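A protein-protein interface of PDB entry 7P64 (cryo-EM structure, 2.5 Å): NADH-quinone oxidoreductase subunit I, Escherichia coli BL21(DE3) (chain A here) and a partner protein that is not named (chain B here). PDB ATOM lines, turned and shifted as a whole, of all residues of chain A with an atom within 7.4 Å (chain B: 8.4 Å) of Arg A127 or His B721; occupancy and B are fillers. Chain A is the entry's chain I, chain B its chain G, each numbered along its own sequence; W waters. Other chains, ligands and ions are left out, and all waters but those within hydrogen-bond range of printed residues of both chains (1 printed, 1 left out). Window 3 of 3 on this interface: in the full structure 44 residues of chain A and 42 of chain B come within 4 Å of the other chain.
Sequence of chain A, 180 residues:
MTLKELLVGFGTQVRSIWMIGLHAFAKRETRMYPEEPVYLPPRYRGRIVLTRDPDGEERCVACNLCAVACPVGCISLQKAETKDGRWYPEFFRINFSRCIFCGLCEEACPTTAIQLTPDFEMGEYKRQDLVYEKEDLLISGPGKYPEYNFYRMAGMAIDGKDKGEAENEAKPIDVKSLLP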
ATOM      1  N   ASN A  95     -31.001 -10.816  -3.917  1.00  0.00           N
ATOM      2  CA  ASN A  95     -30.759 -10.073  -2.685  1.00  0.00           C
ATOM      3  C   ASN A  95     -31.814 -10.500  -1.675  1.00  0.00           C
ATOM      4  O   ASN A  95     -32.929  -9.982  -1.650  1.00  0.00           O
ATOM      5  CB  ASN A  95     -30.794  -8.574  -2.953  1.00  0.00           C
ATOM      6  CG  ASN A  95     -30.316  -7.751  -1.777  1.00  0.00           C
ATOM      7  OD1 ASN A  95     -29.909  -8.284  -0.751  1.00  0.00           O
ATOM      8  ND2 ASN A  95     -30.360  -6.439  -1.926  1.00  0.00           N
ATOM      9  N   PHE A  96     -31.456 -11.463  -0.825  1.00  0.00           N
ATOM     10  CA  PHE A  96     -32.412 -11.982   0.146  1.00  0.00           C
ATOM     11  C   PHE A  96     -32.636 -11.032   1.310  1.00  0.00           C
ATOM     12  O   PHE A  96     -33.606 -11.206   2.051  1.00  0.00           O
ATOM     13  CB  PHE A  96     -31.959 -13.344   0.663  1.00  0.00           C
ATOM     14  CG  PHE A  96     -32.356 -14.482  -0.221  1.00  0.00           C
ATOM     15  CD1 PHE A  96     -33.689 -14.756  -0.461  1.00  0.00           C
ATOM     16  CD2 PHE A  96     -31.400 -15.272  -0.824  1.00  0.00           C
ATOM     17  CE1 PHE A  96     -34.056 -15.800  -1.280  1.00  0.00           C
ATOM     18  CE2 PHE A  96     -31.760 -16.316  -1.641  1.00  0.00           C
ATOM     19  CZ  PHE A  96     -33.087 -16.580  -1.870  1.00  0.00           C
ATOM     20  N   SER A  97     -31.770 -10.034   1.489  1.00  0.00           N
ATOM     21  CA  SER A  97     -32.055  -8.987   2.460  1.00  0.00           C
ATOM     22  C   SER A  97     -33.211  -8.106   2.017  1.00  0.00           C
ATOM     23  O   SER A  97     -33.843  -7.466   2.859  1.00  0.00           O
ATOM     24  CB  SER A  97     -30.807  -8.141   2.711  1.00  0.00           C
ATOM     25  OG  SER A  97     -30.601  -7.193   1.682  1.00  0.00           O
ATOM     26  N   ARG A  98     -33.505  -8.073   0.717  1.00  0.00           N
ATOM     27  CA  ARG A  98     -34.627  -7.322   0.174  1.00  0.00           C
ATOM     28  C   ARG A  98     -35.856  -8.177  -0.088  1.00  0.00           C
ATOM     29  O   ARG A  98     -36.966  -7.639  -0.100  1.00  0.00           O
ATOM     30  CB  ARG A  98     -34.224  -6.642  -1.139  1.00  0.00           C
ATOM     31  CG  ARG A  98     -33.440  -5.367  -0.976  1.00  0.00           C
ATOM     32  CD  ARG A  98     -34.359  -4.177  -0.870  1.00  0.00           C
ATOM     33  NE  ARG A  98     -33.624  -2.922  -0.894  1.00  0.00           N
ATOM     34  CZ  ARG A  98     -34.172  -1.733  -0.702  1.00  0.00           C
ATOM     35  NH1 ARG A  98     -35.465  -1.599  -0.465  1.00  0.00           N
ATOM     36  NH2 ARG A  98     -33.404  -0.651  -0.745  1.00  0.00           N
ATOM     37  N   GLU A 124     -28.416 -14.562   9.184  1.00  0.00           N
ATOM     38  CA  GLU A 124     -27.099 -14.216   8.678  1.00  0.00           C
ATOM     39  C   GLU A 124     -26.454 -13.193   9.599  1.00  0.00           C
ATOM     40  O   GLU A 124     -27.142 -12.421  10.269  1.00  0.00           O
ATOM     41  CB  GLU A 124     -27.198 -13.667   7.250  1.00  0.00           C
ATOM     42  CG  GLU A 124     -25.941 -13.806   6.434  1.00  0.00           C
ATOM     43  CD  GLU A 124     -25.522 -15.244   6.233  1.00  0.00           C
ATOM     44  OE1 GLU A 124     -26.185 -15.952   5.449  1.00  0.00           O
ATOM     45  OE2 GLU A 124     -24.529 -15.662   6.860  1.00  0.00           O
ATOM     46  N   TYR A 125     -25.125 -13.192   9.619  1.00  0.00           N
ATOM     47  CA  TYR A 125     -24.366 -12.256  10.436  1.00  0.00           C
ATOM     48  C   TYR A 125     -24.077 -10.949   9.710  1.00  0.00           C
ATOM     49  O   TYR A 125     -24.187  -9.874  10.307  1.00  0.00           O
ATOM     50  CB  TYR A 125     -23.058 -12.901  10.887  1.00  0.00           C
ATOM     51  CG  TYR A 125     -23.251 -14.017  11.878  1.00  0.00           C
ATOM     52  CD1 TYR A 125     -23.791 -13.770  13.131  1.00  0.00           C
ATOM     53  CD2 TYR A 125     -22.909 -15.321  11.558  1.00  0.00           C
ATOM     54  CE1 TYR A 125     -23.972 -14.789  14.039  1.00  0.00           C
ATOM     55  CE2 TYR A 125     -23.087 -16.345  12.460  1.00  0.00           C
ATOM     56  CZ  TYR A 125     -23.618 -16.071  13.699  1.00  0.00           C
ATOM     57  OH  TYR A 125     -23.799 -17.089  14.601  1.00  0.00           O
ATOM     58  N   LYS A 126     -23.713 -11.016   8.435  1.00  0.00           N
ATOM     59  CA  LYS A 126     -23.436  -9.840   7.628  1.00  0.00           C
ATOM     60  C   LYS A 126     -24.450  -9.756   6.500  1.00  0.00           C
ATOM     61  O   LYS A 126     -24.824 -10.775   5.916  1.00  0.00           O
ATOM     62  CB  LYS A 126     -22.019  -9.875   7.052  1.00  0.00           C
ATOM     63  CG  LYS A 126     -20.952 -10.237   8.059  1.00  0.00           C
ATOM     64  CD  LYS A 126     -20.416  -9.001   8.751  1.00  0.00           C
ATOM     65  CE  LYS A 126     -19.673  -9.362  10.024  1.00  0.00           C
ATOM     66  NZ  LYS A 126     -18.479 -10.208   9.751  1.00  0.00           N
ATOM     67  N   ARG A 127     -24.895  -8.536   6.198  1.00  0.00           N
ATOM     68  CA  ARG A 127     -25.902  -8.347   5.163  1.00  0.00           C
ATOM     69  C   ARG A 127     -25.377  -8.651   3.769  1.00  0.00           C
ATOM     70  O   ARG A 127     -26.171  -8.988   2.887  1.00  0.00           O
ATOM     71  CB  ARG A 127     -26.443  -6.923   5.207  1.00  0.00           C
ATOM     72  CG  ARG A 127     -27.941  -6.850   5.080  1.00  0.00           C
ATOM     73  CD  ARG A 127     -28.412  -5.422   5.002  1.00  0.00           C
ATOM     74  NE  ARG A 127     -28.686  -5.010   3.635  1.00  0.00           N
ATOM     75  CZ  ARG A 127     -28.808  -3.752   3.241  1.00  0.00           C
ATOM     76  NH1 ARG A 127     -28.658  -2.745   4.084  1.00  0.00           N
ATOM     77  NH2 ARG A 127     -29.093  -3.496   1.969  1.00  0.00           N
ATOM     78  N   GLN A 128     -24.064  -8.540   3.553  1.00  0.00           N
ATOM     79  CA  GLN A 128     -23.484  -8.873   2.257  1.00  0.00           C
ATOM     80  C   GLN A 128     -23.638 -10.353   1.931  1.00  0.00           C
ATOM     81  O   GLN A 128     -23.773 -10.718   0.758  1.00  0.00           O
ATOM     82  CB  GLN A 128     -22.009  -8.475   2.230  1.00  0.00           C
ATOM     83  CG  GLN A 128     -21.376  -8.500   0.851  1.00  0.00           C
ATOM     84  CD  GLN A 128     -22.101  -7.619  -0.139  1.00  0.00           C
ATOM     85  OE1 GLN A 128     -22.321  -6.438   0.113  1.00  0.00           O
ATOM     86  NE2 GLN A 128     -22.480  -8.189  -1.273  1.00  0.00           N
ATOM     87  N   ASP A 129     -23.640 -11.213   2.947  1.00  0.00           N
ATOM     88  CA  ASP A 129     -23.795 -12.645   2.742  1.00  0.00           C
ATOM     89  C   ASP A 129     -25.227 -13.052   2.420  1.00  0.00           C
ATOM     90  O   ASP A 129     -25.461 -14.223   2.107  1.00  0.00           O
ATOM     91  CB  ASP A 129     -23.307 -13.408   3.973  1.00  0.00           C
ATOM     92  CG  ASP A 129     -21.876 -13.072   4.333  1.00  0.00           C
ATOM     93  OD1 ASP A 129     -21.062 -12.865   3.410  1.00  0.00           O
ATOM     94  OD2 ASP A 129     -21.562 -13.012   5.540  1.00  0.00           O
ATOM     95  N   LEU A 130     -26.183 -12.131   2.492  1.00  0.00           N
ATOM     96  CA  LEU A 130     -27.547 -12.406   2.067  1.00  0.00           C
ATOM     97  C   LEU A 130     -27.741 -12.241   0.567  1.00  0.00           C
ATOM     98  O   LEU A 130     -28.846 -12.471   0.073  1.00  0.00           O
ATOM     99  CB  LEU A 130     -28.525 -11.505   2.822  1.00  0.00           C
ATOM    100  CG  LEU A 130     -28.842 -11.963   4.244  1.00  0.00           C
ATOM    101  CD1 LEU A 130     -29.786 -10.995   4.923  1.00  0.00           C
ATOM    102  CD2 LEU A 130     -29.420 -13.365   4.233  1.00  0.00           C
ATOM    103  N   VAL A 131     -26.709 -11.838  -0.164  1.00  0.00           N
ATOM    104  CA  VAL A 131     -26.742 -11.826  -1.621  1.00  0.00           C
ATOM    105  C   VAL A 131     -26.326 -13.213  -2.089  1.00  0.00           C
ATOM    106  O   VAL A 131     -25.155 -13.586  -1.995  1.00  0.00           O
ATOM    107  CB  VAL A 131     -25.829 -10.742  -2.201  1.00  0.00           C
ATOM    108  CG1 VAL A 131     -25.878 -10.769  -3.718  1.00  0.00           C
ATOM    109  CG2 VAL A 131     -26.234  -9.383  -1.680  1.00  0.00           C
ATOM    110  N   TYR B 637     -21.519   4.263 -12.359  1.00  0.00           N
ATOM    111  CA  TYR B 637     -22.542   3.628 -11.536  1.00  0.00           C
ATOM    112  C   TYR B 637     -22.096   2.255 -11.052  1.00  0.00           C
ATOM    113  O   TYR B 637     -22.285   1.916  -9.880  1.00  0.00           O
ATOM    114  CB  TYR B 637     -23.851   3.526 -12.314  1.00  0.00           C
ATOM    115  CG  TYR B 637     -24.985   2.923 -11.521  1.00  0.00           C
ATOM    116  CD1 TYR B 637     -25.656   3.664 -10.561  1.00  0.00           C
ATOM    117  CD2 TYR B 637     -25.381   1.609 -11.731  1.00  0.00           C
ATOM    118  CE1 TYR B 637     -26.691   3.117  -9.835  1.00  0.00           C
ATOM    119  CE2 TYR B 637     -26.412   1.053 -11.009  1.00  0.00           C
ATOM    120  CZ  TYR B 637     -27.064   1.810 -10.064  1.00  0.00           C
ATOM    121  OH  TYR B 637     -28.095   1.254  -9.344  1.00  0.00           O
ATOM    122  N   ARG B 711     -33.386  -3.405  -9.463  1.00  0.00           N
ATOM    123  CA  ARG B 711     -32.780  -2.181  -8.948  1.00  0.00           C
ATOM    124  C   ARG B 711     -32.087  -2.399  -7.609  1.00  0.00           C
ATOM    125  O   ARG B 711     -31.134  -1.683  -7.288  1.00  0.00           O
ATOM    126  CB  ARG B 711     -33.829  -1.081  -8.832  1.00  0.00           C
ATOM    127  CG  ARG B 711     -35.027  -1.414  -7.963  1.00  0.00           C
ATOM    128  CD  ARG B 711     -36.293  -0.567  -8.231  1.00  0.00           C
ATOM    129  NE  ARG B 711     -36.211   0.832  -7.819  1.00  0.00           N
ATOM    130  CZ  ARG B 711     -35.638   1.809  -8.512  1.00  0.00           C
ATOM    131  NH1 ARG B 711     -35.246   1.638  -9.764  1.00  0.00           N
ATOM    132  NH2 ARG B 711     -35.491   3.002  -7.948  1.00  0.00           N
ATOM    133  N   THR B 712     -32.531  -3.376  -6.823  1.00  0.00           N
ATOM    134  CA  THR B 712     -31.880  -3.695  -5.561  1.00  0.00           C
ATOM    135  C   THR B 712     -30.968  -4.910  -5.666  1.00  0.00           C
ATOM    136  O   THR B 712     -30.536  -5.435  -4.637  1.00  0.00           O
ATOM    137  CB  THR B 712     -32.920  -3.910  -4.457  1.00  0.00           C
ATOM    138  OG1 THR B 712     -33.732  -5.046  -4.764  1.00  0.00           O
ATOM    139  CG2 THR B 712     -33.804  -2.687  -4.314  1.00  0.00           C
ATOM    140  N   ARG B 715     -26.384  -4.242  -8.603  1.00  0.00           N
ATOM    141  CA  ARG B 715     -25.086  -3.890  -8.045  1.00  0.00           C
ATOM    142  C   ARG B 715     -24.856  -4.548  -6.691  1.00  0.00           C
ATOM    143  O   ARG B 715     -23.960  -4.138  -5.950  1.00  0.00           O
ATOM    144  CB  ARG B 715     -24.964  -2.372  -7.927  1.00  0.00           C
ATOM    145  CG  ARG B 715     -23.595  -1.827  -8.251  1.00  0.00           C
ATOM    146  CD  ARG B 715     -23.535  -0.357  -7.913  1.00  0.00           C
ATOM    147  NE  ARG B 715     -22.170   0.149  -7.865  1.00  0.00           N
ATOM    148  CZ  ARG B 715     -21.460   0.281  -6.754  1.00  0.00           C
ATOM    149  NH1 ARG B 715     -21.957  -0.047  -5.573  1.00  0.00           N
ATOM    150  NH2 ARG B 715     -20.220   0.754  -6.831  1.00  0.00           N
ATOM    151  N   ALA B 716     -25.649  -5.568  -6.355  1.00  0.00           N
ATOM    152  CA  ALA B 716     -25.611  -6.147  -5.019  1.00  0.00           C
ATOM    153  C   ALA B 716     -24.359  -6.976  -4.766  1.00  0.00           C
ATOM    154  O   ALA B 716     -24.013  -7.205  -3.604  1.00  0.00           O
ATOM    155  CB  ALA B 716     -26.854  -7.001  -4.779  1.00  0.00           C
ATOM    156  N   ASN B 717     -23.673  -7.433  -5.815  1.00  0.00           N
ATOM    157  CA  ASN B 717     -22.445  -8.188  -5.600  1.00  0.00           C
ATOM    158  C   ASN B 717     -21.294  -7.280  -5.183  1.00  0.00           C
ATOM    159  O   ASN B 717     -20.415  -7.708  -4.427  1.00  0.00           O
ATOM    160  CB  ASN B 717     -22.071  -8.975  -6.854  1.00  0.00           C
ATOM    161  CG  ASN B 717     -21.931  -8.097  -8.072  1.00  0.00           C
ATOM    162  OD1 ASN B 717     -22.669  -7.130  -8.244  1.00  0.00           O
ATOM    163  ND2 ASN B 717     -20.969  -8.420  -8.924  1.00  0.00           N
ATOM    164  N   ILE B 718     -21.269  -6.040  -5.672  1.00  0.00           N
ATOM    165  CA  ILE B 718     -20.249  -5.091  -5.235  1.00  0.00           C
ATOM    166  C   ILE B 718     -20.516  -4.655  -3.800  1.00  0.00           C
ATOM    167  O   ILE B 718     -19.622  -4.680  -2.948  1.00  0.00           O
ATOM    168  CB  ILE B 718     -20.186  -3.890  -6.196  1.00  0.00           C
ATOM    169  CG1 ILE B 718     -19.600  -4.319  -7.539  1.00  0.00           C
ATOM    170  CG2 ILE B 718     -19.352  -2.765  -5.605  1.00  0.00           C
ATOM    171  CD1 ILE B 718     -20.561  -4.201  -8.677  1.00  0.00           C
ATOM    172  N   SER B 719     -21.755  -4.265  -3.510  1.00  0.00           N
ATOM    173  CA  SER B 719     -22.167  -3.959  -2.149  1.00  0.00           C
ATOM    174  C   SER B 719     -23.675  -4.124  -2.054  1.00  0.00           C
ATOM    175  O   SER B 719     -24.403  -3.765  -2.980  1.00  0.00           O
ATOM    176  CB  SER B 719     -21.764  -2.542  -1.731  1.00  0.00           C
ATOM    177  OG  SER B 719     -22.633  -1.578  -2.287  1.00  0.00           O
ATOM    178  N   VAL B 720     -24.133  -4.664  -0.923  1.00  0.00           N
ATOM    179  CA  VAL B 720     -25.560  -4.850  -0.703  1.00  0.00           C
ATOM    180  C   VAL B 720     -26.270  -3.517  -0.492  1.00  0.00           C
ATOM    181  O   VAL B 720     -27.489  -3.431  -0.670  1.00  0.00           O
ATOM    182  CB  VAL B 720     -25.776  -5.825   0.475  1.00  0.00           C
ATOM    183  CG1 VAL B 720     -25.516  -5.144   1.808  1.00  0.00           C
ATOM    184  CG2 VAL B 720     -27.167  -6.441   0.430  1.00  0.00           C
ATOM    185  N   HIS B 721     -25.536  -2.463  -0.148  1.00  0.00           N
ATOM    186  CA  HIS B 721     -26.121  -1.137  -0.029  1.00  0.00           C
ATOM    187  C   HIS B 721     -26.322  -0.535  -1.413  1.00  0.00           C
ATOM    188  O   HIS B 721     -25.380  -0.451  -2.204  1.00  0.00           O
ATOM    189  CB  HIS B 721     -25.225  -0.241   0.821  1.00  0.00           C
ATOM    190  CG  HIS B 721     -25.051  -0.728   2.223  1.00  0.00           C
ATOM    191  ND1 HIS B 721     -25.955  -0.449   3.224  1.00  0.00           N
ATOM    192  CD2 HIS B 721     -24.087  -1.492   2.788  1.00  0.00           C
ATOM    193  CE1 HIS B 721     -25.551  -1.011   4.348  1.00  0.00           C
ATOM    194  NE2 HIS B 721     -24.421  -1.650   4.110  1.00  0.00           N
ATOM    195  N   GLU B 722     -27.554  -0.127  -1.702  1.00  0.00           N
ATOM    196  CA  GLU B 722     -27.862   0.434  -3.007  1.00  0.00           C
ATOM    197  C   GLU B 722     -27.179   1.789  -3.173  1.00  0.00           C
ATOM    198  O   GLU B 722     -27.184   2.606  -2.250  1.00  0.00           O
ATOM    199  CB  GLU B 722     -29.371   0.584  -3.193  1.00  0.00           C
ATOM    200  CG  GLU B 722     -30.102  -0.723  -3.421  1.00  0.00           C
ATOM    201  CD  GLU B 722     -30.555  -1.365  -2.125  1.00  0.00           C
ATOM    202  OE1 GLU B 722     -30.648  -0.646  -1.109  1.00  0.00           O
ATOM    203  OE2 GLU B 722     -30.811  -2.584  -2.119  1.00  0.00           O
ATOM    204  N   PRO B 723     -26.581   2.051  -4.327  1.00  0.00           N
ATOM    205  CA  PRO B 723     -25.877   3.315  -4.534  1.00  0.00           C
ATOM    206  C   PRO B 723     -26.847   4.460  -4.788  1.00  0.00           C
ATOM    207  O   PRO B 723     -28.038   4.269  -5.031  1.00  0.00           O
ATOM    208  CB  PRO B 723     -25.022   3.030  -5.767  1.00  0.00           C
ATOM    209  CG  PRO B 723     -25.836   2.063  -6.532  1.00  0.00           C
ATOM    210  CD  PRO B 723     -26.524   1.191  -5.520  1.00  0.00           C
ATOM    211  N   ARG B 724     -26.302   5.670  -4.711  1.00  0.00           N
ATOM    212  CA  ARG B 724     -27.071   6.876  -4.986  1.00  0.00           C
ATOM    213  C   ARG B 724     -27.415   6.897  -6.475  1.00  0.00           C
ATOM    214  O   ARG B 724     -26.569   6.585  -7.318  1.00  0.00           O
ATOM    215  CB  ARG B 724     -26.241   8.098  -4.550  1.00  0.00           C
ATOM    216  CG  ARG B 724     -26.930   9.467  -4.259  1.00  0.00           C
ATOM    217  CD  ARG B 724     -27.778  10.044  -5.369  1.00  0.00           C
ATOM    218  NE  ARG B 724     -28.024  11.476  -5.252  1.00  0.00           N
ATOM    219  CZ  ARG B 724     -29.140  12.007  -4.771  1.00  0.00           C
ATOM    220  NH1 ARG B 724     -30.143  11.250  -4.361  1.00  0.00           N
ATOM    221  NH2 ARG B 724     -29.257  13.330  -4.714  1.00  0.00           N
HETATM  222  O   HOH W   1     -30.541  -1.138   1.418  1.00  0.00           O
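O of Thr B712 lies within hydrogen-bond range of ND2 of Asn A95 (2.9 Å). The side-chain amide oxygen of Gln A128 sits at hydrogen-bond distance from the backbone NH of Val B720, 2.7 Å away. The backbone carbonyl oxygen (O) of Ala B716 is in hydrogen-bond range of the side-chain amide nitrogen (NE2) of Gln A128 (3.0 Å). The guanidinium group (NH2) of Arg A98 is in salt-bridge range of the side-chain carboxylate (OE1) of Glu B722 (2.8 Å). The backbone carbonyl oxygen (O) of Val B720 sits at hydrogen-bond distance from the guanidinium group (NH2) of Arg A127 (3.1 Å).
OD1 of Asn A95 sits at hydrogen-bond distance from OG of Ser A97 (2.8 Å). The side-chain hydroxyl (OG) of Ser B719 is in hydrogen-bond range of the backbone carbonyl oxygen (O) of His B721 (3.0 Å). The guanidinium group of Arg A127 lies within hydrogen-bond range of the side-chain hydroxyl of Ser A97 (3.5 Å).
Val B720 touches Asn A95. Glu B722 touches Asn A95. OG of Ser A97 touches CG2 of Val B720, 3.7 Å away. Thr B712 touches Arg A98 (CG2 to NE, 3.4 Å). NH1 of Arg A127 touches CE1 of His B721 (3.6 Å). Gln A128 touches Asn B717 (NE2 to O, 3.8 Å). Ser B719 touches Gln A128 (CA to OE1, 3.4 Å). Ala B716 touches Val A131. Val B720 touches Val A131 (CG2 to CG2, 3.7 Å).
Phe A96 touches none of the printed residues of chain B. Of the printed residues of chain B, Ser A97 touches Val B720. Printed residues of chain B within 4 Å of Arg A98: Thr B712 (3.4 Å) and Glu B722 (2.8 Å). Arg A127 touches two residues of chain B. Asp A129 touches none of the printed residues of chain B. Of the printed residues of chain A, Thr B712 touches Asn A95 and Arg A98. His B721 touches one residue of chain A.
Hydrophobic or aromatic side chains of chain B within 4 Å of the printed part of chain A: Ala B716, Val B720 and His B721. Hydrophobic or aromatic side chains of chain A within 4 Å of the printed part of chain B: Val A131. Among the printed residues, 14 pairs touch across the chains. Among the printed residues, Asp or Glu carboxylates within 4 Å of a Lys or Arg side-chain nitrogen of the other chain: Arg A98 with Glu B722 (2.8 Å).
Water W1 lies within hydrogen-bond range of the side-chain carboxylate of Glu B722 (2.6 Å) and the guanidinium group of Arg A127 (2.8 Å).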
